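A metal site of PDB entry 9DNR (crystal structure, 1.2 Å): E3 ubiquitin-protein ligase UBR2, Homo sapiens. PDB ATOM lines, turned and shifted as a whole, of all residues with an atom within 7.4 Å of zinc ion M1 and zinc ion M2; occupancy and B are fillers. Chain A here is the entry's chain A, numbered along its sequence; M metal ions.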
ATOM      1  N   LEU A   1      23.420  -3.617   1.530  1.00  0.00           N
ATOM      2  CA  LEU A   1      22.999  -2.445   2.279  1.00  0.00           C
ATOM      3  C   LEU A   1      22.895  -1.208   1.391  1.00  0.00           C
ATOM      4  O   LEU A   1      23.674  -1.016   0.452  1.00  0.00           O
ATOM      5  CB  LEU A   1      23.983  -2.136   3.401  1.00  0.00           C
ATOM      6  CG  LEU A   1      23.762  -2.768   4.766  1.00  0.00           C
ATOM      7  CD1 LEU A   1      24.030  -4.260   4.698  1.00  0.00           C
ATOM      8  CD2 LEU A   1      24.661  -2.093   5.777  1.00  0.00           C
ATOM      9  N   CYS A   2      21.924  -0.356   1.720  1.00  0.00           N
ATOM     10  CA  CYS A   2      21.748   0.906   1.012  1.00  0.00           C
ATOM     11  C   CYS A   2      22.992   1.792   1.089  1.00  0.00           C
ATOM     12  O   CYS A   2      23.642   2.054   0.073  1.00  0.00           O
ATOM     13  CB  CYS A   2      20.549   1.669   1.554  1.00  0.00           C
ATOM     14  SG  CYS A   2      20.351   3.241   0.704  1.00  0.00           S
ATOM     15  N   GLY A   3      23.289   2.282   2.282  1.00  0.00           N
ATOM     16  CA  GLY A   3      24.471   3.078   2.482  1.00  0.00           C
ATOM     17  C   GLY A   3      24.475   4.454   1.854  1.00  0.00           C
ATOM     18  O   GLY A   3      25.513   5.135   1.904  1.00  0.00           O
ATOM     19  N   ARG A   4      23.362   4.893   1.252  1.00  0.00           N
ATOM     20  CA  ARG A   4      23.347   6.141   0.485  1.00  0.00           C
ATOM     21  C   ARG A   4      23.818   7.321   1.323  1.00  0.00           C
ATOM     22  O   ARG A   4      23.321   7.555   2.419  1.00  0.00           O
ATOM     23  CB  ARG A   4      21.942   6.433  -0.059  1.00  0.00           C
ATOM     24  CG  ARG A   4      21.917   7.711  -0.879  1.00  0.00           C
ATOM     25  CD  ARG A   4      20.532   8.245  -1.193  1.00  0.00           C
ATOM     26  NE  ARG A   4      19.720   7.284  -1.939  1.00  0.00           N
ATOM     27  CZ  ARG A   4      18.687   7.629  -2.698  1.00  0.00           C
ATOM     28  NH1 ARG A   4      18.360   8.897  -2.886  1.00  0.00           N
ATOM     29  NH2 ARG A   4      17.953   6.685  -3.278  1.00  0.00           N
ATOM     30  N   PHE A   6      23.725  11.231   1.781  1.00  0.00           N
ATOM     31  CA  PHE A   6      22.798  12.279   1.375  1.00  0.00           C
ATOM     32  C   PHE A   6      23.528  13.436   0.711  1.00  0.00           C
ATOM     33  O   PHE A   6      24.643  13.809   1.104  1.00  0.00           O
ATOM     34  CB  PHE A   6      22.057  12.810   2.581  1.00  0.00           C
ATOM     35  CG  PHE A   6      21.288  11.764   3.271  1.00  0.00           C
ATOM     36  CD1 PHE A   6      20.319  11.031   2.604  1.00  0.00           C
ATOM     37  CD2 PHE A   6      21.547  11.457   4.597  1.00  0.00           C
ATOM     38  CE1 PHE A   6      19.610  10.035   3.248  1.00  0.00           C
ATOM     39  CE2 PHE A   6      20.836  10.472   5.233  1.00  0.00           C
ATOM     40  CZ  PHE A   6      19.877   9.769   4.567  1.00  0.00           C
ATOM     41  N   VAL A  25      17.928   7.726  10.262  1.00  0.00           N
ATOM     42  CA  VAL A  25      17.266   8.293   9.097  1.00  0.00           C
ATOM     43  C   VAL A  25      17.318   7.322   7.927  1.00  0.00           C
ATOM     44  O   VAL A  25      18.168   6.433   7.853  1.00  0.00           O
ATOM     45  CB  VAL A  25      17.915   9.621   8.667  1.00  0.00           C
ATOM     46  CG1 VAL A  25      17.600  10.721   9.685  1.00  0.00           C
ATOM     47  CG2 VAL A  25      19.423   9.432   8.481  1.00  0.00           C
ATOM     48  N   LEU A  26      16.409   7.549   6.970  1.00  0.00           N
ATOM     49  CA  LEU A  26      16.315   6.769   5.745  1.00  0.00           C
ATOM     50  C   LEU A  26      16.309   7.718   4.571  1.00  0.00           C
ATOM     51  O   LEU A  26      15.754   8.824   4.643  1.00  0.00           O
ATOM     52  CB  LEU A  26      15.010   5.971   5.693  1.00  0.00           C
ATOM     53  CG  LEU A  26      14.838   4.914   6.771  1.00  0.00           C
ATOM     54  CD1 LEU A  26      13.435   4.326   6.712  1.00  0.00           C
ATOM     55  CD2 LEU A  26      15.866   3.821   6.619  1.00  0.00           C
ATOM     56  N   CYS A  27      16.913   7.277   3.460  1.00  0.00           N
ATOM     57  CA  CYS A  27      16.768   7.964   2.179  1.00  0.00           C
ATOM     58  C   CYS A  27      15.349   7.760   1.649  1.00  0.00           C
ATOM     59  O   CYS A  27      14.564   6.955   2.162  1.00  0.00           O
ATOM     60  CB  CYS A  27      17.784   7.427   1.178  1.00  0.00           C
ATOM     61  SG  CYS A  27      17.430   5.760   0.521  1.00  0.00           S
ATOM     62  N   MET A  28      15.010   8.496   0.599  1.00  0.00           N
ATOM     63  CA  MET A  28      13.624   8.465   0.134  1.00  0.00           C
ATOM     64  C   MET A  28      13.259   7.100  -0.420  1.00  0.00           C
ATOM     65  O   MET A  28      12.129   6.635  -0.220  1.00  0.00           O
ATOM     66  CB  MET A  28      13.371   9.539  -0.919  1.00  0.00           C
ATOM     67  CG  MET A  28      14.125   9.340  -2.188  1.00  0.00           C
ATOM     68  SD  MET A  28      13.793  10.629  -3.375  1.00  0.00           S
ATOM     69  CE  MET A  28      14.018  12.048  -2.324  1.00  0.00           C
ATOM     70  N   GLU A  29      14.190   6.427  -1.093  1.00  0.00           N
ATOM     71  CA  GLU A  29      13.852   5.124  -1.666  1.00  0.00           C
ATOM     72  C   GLU A  29      13.547   4.116  -0.561  1.00  0.00           C
ATOM     73  O   GLU A  29      12.563   3.362  -0.638  1.00  0.00           O
ATOM     74  CB  GLU A  29      15.037   4.674  -2.525  1.00  0.00           C
ATOM     75  CG  GLU A  29      14.933   3.272  -3.040  1.00  0.00           C
ATOM     76  CD  GLU A  29      16.202   2.823  -3.731  1.00  0.00           C
ATOM     77  OE1 GLU A  29      17.261   3.472  -3.564  1.00  0.00           O
ATOM     78  OE2 GLU A  29      16.119   1.810  -4.449  1.00  0.00           O
ATOM     79  N   CYS A  30      14.372   4.111   0.485  1.00  0.00           N
ATOM     80  CA  CYS A  30      14.135   3.166   1.572  1.00  0.00           C
ATOM     81  C   CYS A  30      12.888   3.519   2.367  1.00  0.00           C
ATOM     82  O   CYS A  30      12.076   2.649   2.684  1.00  0.00           O
ATOM     83  CB  CYS A  30      15.377   3.064   2.432  1.00  0.00           C
ATOM     84  SG  CYS A  30      16.797   2.412   1.494  1.00  0.00           S
ATOM     85  N   PHE A  31      12.702   4.803   2.661  1.00  0.00           N
ATOM     86  CA  PHE A  31      11.516   5.224   3.386  1.00  0.00           C
ATOM     87  C   PHE A  31      10.234   4.788   2.659  1.00  0.00           C
ATOM     88  O   PHE A  31       9.336   4.199   3.260  1.00  0.00           O
ATOM     89  CB  PHE A  31      11.539   6.731   3.589  1.00  0.00           C
ATOM     90  CG  PHE A  31      10.245   7.275   4.067  1.00  0.00           C
ATOM     91  CD1 PHE A  31       9.860   7.066   5.368  1.00  0.00           C
ATOM     92  CD2 PHE A  31       9.413   7.991   3.225  1.00  0.00           C
ATOM     93  CE1 PHE A  31       8.639   7.553   5.837  1.00  0.00           C
ATOM     94  CE2 PHE A  31       8.202   8.496   3.690  1.00  0.00           C
ATOM     95  CZ  PHE A  31       7.817   8.274   4.985  1.00  0.00           C
ATOM     96  N   GLY A  33       9.743   2.441   0.588  1.00  0.00           N
ATOM     97  CA  GLY A  33       9.600   1.000   0.575  1.00  0.00           C
ATOM     98  C   GLY A  33       9.592   0.378   1.957  1.00  0.00           C
ATOM     99  O   GLY A  33       9.751  -0.845   2.070  1.00  0.00           O
ATOM    100  N   SER A  34       9.394   1.159   3.010  1.00  0.00           N
ATOM    101  CA  SER A  34       9.467   0.661   4.369  1.00  0.00           C
ATOM    102  C   SER A  34       8.092   0.730   5.036  1.00  0.00           C
ATOM    103  O   SER A  34       7.143   1.336   4.552  1.00  0.00           O
ATOM    104  CB  SER A  34      10.446   1.489   5.217  1.00  0.00           C
ATOM    105  OG  SER A  34       9.893   2.745   5.591  1.00  0.00           O
ATOM    106  N   PHE A  51      24.214   9.477   6.179  1.00  0.00           N
ATOM    107  CA  PHE A  51      23.925   8.311   5.348  1.00  0.00           C
ATOM    108  C   PHE A  51      22.640   7.629   5.797  1.00  0.00           C
ATOM    109  O   PHE A  51      22.213   7.753   6.955  1.00  0.00           O
ATOM    110  CB  PHE A  51      25.084   7.317   5.292  1.00  0.00           C
ATOM    111  CG  PHE A  51      25.507   6.786   6.625  1.00  0.00           C
ATOM    112  CD1 PHE A  51      24.912   5.635   7.144  1.00  0.00           C
ATOM    113  CD2 PHE A  51      26.474   7.436   7.384  1.00  0.00           C
ATOM    114  CE1 PHE A  51      25.282   5.150   8.385  1.00  0.00           C
ATOM    115  CE2 PHE A  51      26.843   6.950   8.624  1.00  0.00           C
ATOM    116  CZ  PHE A  51      26.256   5.802   9.121  1.00  0.00           C
ATOM    117  N   CYS A  52      22.065   6.866   4.872  1.00  0.00           N
ATOM    118  CA  CYS A  52      20.862   6.106   5.139  1.00  0.00           C
ATOM    119  C   CYS A  52      21.149   4.937   6.070  1.00  0.00           C
ATOM    120  O   CYS A  52      22.129   4.195   5.883  1.00  0.00           O
ATOM    121  CB  CYS A  52      20.304   5.608   3.813  1.00  0.00           C
ATOM    122  SG  CYS A  52      18.830   4.598   3.998  1.00  0.00           S
ATOM    123  N   ASP A  53      20.272   4.754   7.058  1.00  0.00           N
ATOM    124  CA  ASP A  53      20.398   3.708   8.061  1.00  0.00           C
ATOM    125  C   ASP A  53      19.559   2.462   7.750  1.00  0.00           C
ATOM    126  O   ASP A  53      19.325   1.650   8.658  1.00  0.00           O
ATOM    127  CB  ASP A  53      20.012   4.235   9.431  1.00  0.00           C
ATOM    128  CG  ASP A  53      20.946   5.319   9.895  1.00  0.00           C
ATOM    129  OD1 ASP A  53      22.181   5.111   9.861  1.00  0.00           O
ATOM    130  OD2 ASP A  53      20.454   6.404  10.242  1.00  0.00           O
ATOM    131  N   CYS A  54      19.119   2.304   6.510  1.00  0.00           N
ATOM    132  CA  CYS A  54      18.385   1.085   6.172  1.00  0.00           C
ATOM    133  C   CYS A  54      19.242  -0.138   6.461  1.00  0.00           C
ATOM    134  O   CYS A  54      20.406  -0.214   6.051  1.00  0.00           O
ATOM    135  CB  CYS A  54      17.971   1.107   4.700  1.00  0.00           C
ATOM    136  SG  CYS A  54      17.151  -0.388   4.176  1.00  0.00           S
ATOM    137  N   GLY A  55      18.654  -1.091   7.190  1.00  0.00           N
ATOM    138  CA  GLY A  55      19.336  -2.311   7.563  1.00  0.00           C
ATOM    139  C   GLY A  55      19.910  -2.348   8.962  1.00  0.00           C
ATOM    140  O   GLY A  55      20.319  -3.426   9.414  1.00  0.00           O
ATOM    141  N   PRO A  64      13.659  -2.524  10.333  1.00  0.00           N
ATOM    142  CA  PRO A  64      14.987  -1.961   9.988  1.00  0.00           C
ATOM    143  C   PRO A  64      15.299  -1.938   8.508  1.00  0.00           C
ATOM    144  O   PRO A  64      16.017  -1.031   8.062  1.00  0.00           O
ATOM    145  CB  PRO A  64      15.969  -2.862  10.762  1.00  0.00           C
ATOM    146  CG  PRO A  64      15.220  -4.160  10.914  1.00  0.00           C
ATOM    147  CD  PRO A  64      13.782  -3.772  11.119  1.00  0.00           C
ATOM    148  N   TYR A  65      14.771  -2.860   7.729  1.00  0.00           N
ATOM    149  CA  TYR A  65      15.009  -2.938   6.289  1.00  0.00           C
ATOM    150  C   TYR A  65      13.768  -2.512   5.513  1.00  0.00           C
ATOM    151  O   TYR A  65      12.637  -2.703   5.978  1.00  0.00           O
ATOM    152  CB  TYR A  65      15.338  -4.370   5.872  1.00  0.00           C
ATOM    153  CG  TYR A  65      16.722  -4.843   6.243  1.00  0.00           C
ATOM    154  CD1 TYR A  65      16.970  -5.461   7.470  1.00  0.00           C
ATOM    155  CD2 TYR A  65      17.783  -4.695   5.362  1.00  0.00           C
ATOM    156  CE1 TYR A  65      18.234  -5.922   7.792  1.00  0.00           C
ATOM    157  CE2 TYR A  65      19.057  -5.153   5.675  1.00  0.00           C
ATOM    158  CZ  TYR A  65      19.279  -5.758   6.890  1.00  0.00           C
ATOM    159  OH  TYR A  65      20.546  -6.200   7.202  1.00  0.00           O
ATOM    160  N   CYS A  66      13.989  -1.943   4.338  1.00  0.00           N
ATOM    161  CA  CYS A  66      12.942  -1.684   3.376  1.00  0.00           C
ATOM    162  C   CYS A  66      12.788  -2.889   2.458  1.00  0.00           C
ATOM    163  O   CYS A  66      13.569  -3.852   2.505  1.00  0.00           O
ATOM    164  CB  CYS A  66      13.259  -0.427   2.558  1.00  0.00           C
ATOM    165  SG  CYS A  66      14.512  -0.703   1.297  1.00  0.00           S
ATOM    166  N   GLN A  67      11.781  -2.821   1.589  1.00  0.00           N
ATOM    167  CA  GLN A  67      11.488  -3.965   0.741  1.00  0.00           C
ATOM    168  C   GLN A  67      12.598  -4.261  -0.251  1.00  0.00           C
ATOM    169  O   GLN A  67      12.762  -5.419  -0.668  1.00  0.00           O
ATOM    170  CB  GLN A  67      10.142  -3.778   0.043  1.00  0.00           C
ATOM    171  CG  GLN A  67      10.149  -2.797  -1.115  1.00  0.00           C
ATOM    172  CD  GLN A  67       8.757  -2.274  -1.441  1.00  0.00           C
ATOM    173  OE1 GLN A  67       7.782  -2.613  -0.763  1.00  0.00           O
ATOM    174  NE2 GLN A  67       8.646  -1.472  -2.498  1.00  0.00           N
ATOM    175  N   LYS A  68      13.391  -3.251  -0.629  1.00  0.00           N
ATOM    176  CA  LYS A  68      14.467  -3.440  -1.602  1.00  0.00           C
ATOM    177  C   LYS A  68      15.682  -4.113  -0.989  1.00  0.00           C
ATOM    178  O   LYS A  68      16.380  -4.886  -1.664  1.00  0.00           O
ATOM    179  CB  LYS A  68      14.884  -2.087  -2.152  1.00  0.00           C
ATOM    180  CG  LYS A  68      16.128  -2.160  -3.015  1.00  0.00           C
ATOM    181  CD  LYS A  68      16.230  -0.954  -3.880  1.00  0.00           C
ATOM    182  CE  LYS A  68      17.504  -0.997  -4.687  1.00  0.00           C
ATOM    183  NZ  LYS A  68      17.575   0.174  -5.578  1.00  0.00           N
ATOM    184  N   HIS A  69      15.976  -3.829   0.276  1.00  0.00           N
ATOM    185  CA  HIS A  69      17.219  -4.287   0.869  1.00  0.00           C
ATOM    186  C   HIS A  69      17.040  -5.478   1.808  1.00  0.00           C
ATOM    187  O   HIS A  69      18.047  -6.097   2.177  1.00  0.00           O
ATOM    188  CB  HIS A  69      17.924  -3.113   1.557  1.00  0.00           C
ATOM    189  CG  HIS A  69      18.336  -2.053   0.587  1.00  0.00           C
ATOM    190  ND1 HIS A  69      17.817  -0.782   0.594  1.00  0.00           N
ATOM    191  CD2 HIS A  69      19.166  -2.120  -0.482  1.00  0.00           C
ATOM    192  CE1 HIS A  69      18.358  -0.084  -0.388  1.00  0.00           C
ATOM    193  NE2 HIS A  69      19.175  -0.879  -1.063  1.00  0.00           N
ATOM    194  N   GLU A  70      15.809  -5.811   2.170  1.00  0.00           N
ATOM    195  CA  GLU A  70      15.523  -6.966   3.041  1.00  0.00           C
ATOM    196  C   GLU A  70      16.006  -8.285   2.426  1.00  0.00           C
ATOM    197  O   GLU A  70      16.323  -9.218   3.174  1.00  0.00           O
ATOM    198  CB  GLU A  70      14.018  -7.091   3.358  1.00  0.00           C
ATOM    199  CG  GLU A  70      13.139  -7.421   2.158  1.00  0.00           C
ATOM    200  CD  GLU A  70      11.646  -7.400   2.473  1.00  0.00           C
ATOM    201  OE1 GLU A  70      11.293  -7.487   3.665  1.00  0.00           O
ATOM    202  OE2 GLU A  70      10.821  -7.297   1.543  1.00  0.00           O
ATOM    203  OXT GLU A  70      16.051  -8.448   1.207  1.00  0.00           O
HETATM  204 ZN    ZN M   1      16.592   0.120   1.986  1.00  0.00          ZN
HETATM  205 ZN    ZN M   2      18.474   4.087   1.741  1.00  0.00          ZN
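N of Cys 52 sits at hydrogen-bond distance from O of Arg 4. The backbone NH (N) of Arg 4 sits close to the side-chain sulfur (SG) of Cys 2 (3.5 Å). The backbone NH of Cys 54 lies close to the side-chain sulfur of Cys 52, at 3.4 Å. SG of Cys 27 sits close to NE of Arg 4, 3.7 Å away. N of Glu 29 sits close to SG of Cys 27 (3.7 Å). The backbone NH (N) of Lys 68 lies close to the side-chain sulfur (SG) of Cys 66, at 3.4 Å.
Within 4 Å of zinc ion M1: Cys 30, Cys 54, Cys 66 and His 69. The nearest printed residue that does not touch zinc ion M1 is Cys 2 (4.3 Å).
Within 4 Å of zinc ion M2: Cys 2, Cys 27, Cys 30 and Cys 52. The nearest printed residue that does not touch zinc ion M2 is Cys 54 (4.2 Å).
Zinc ion M1 is bound by a ring nitrogen (ND1) of His 69 (2.1 Å), the side-chain sulfur (SG) of Cys 54 (2.3 Å), the side-chain sulfur (SG) of Cys 66 (2.3 Å) and the side-chain sulfur (SG) of Cys 30 (2.4 Å).
SG of Cys 2 binds zinc ion M2. Zinc ion M2 is bound by SG of Cys 27. SG of Cys 52 is bound to zinc ion M2. SG of Cys 30 binds zinc ion M2 (2.4 Å).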
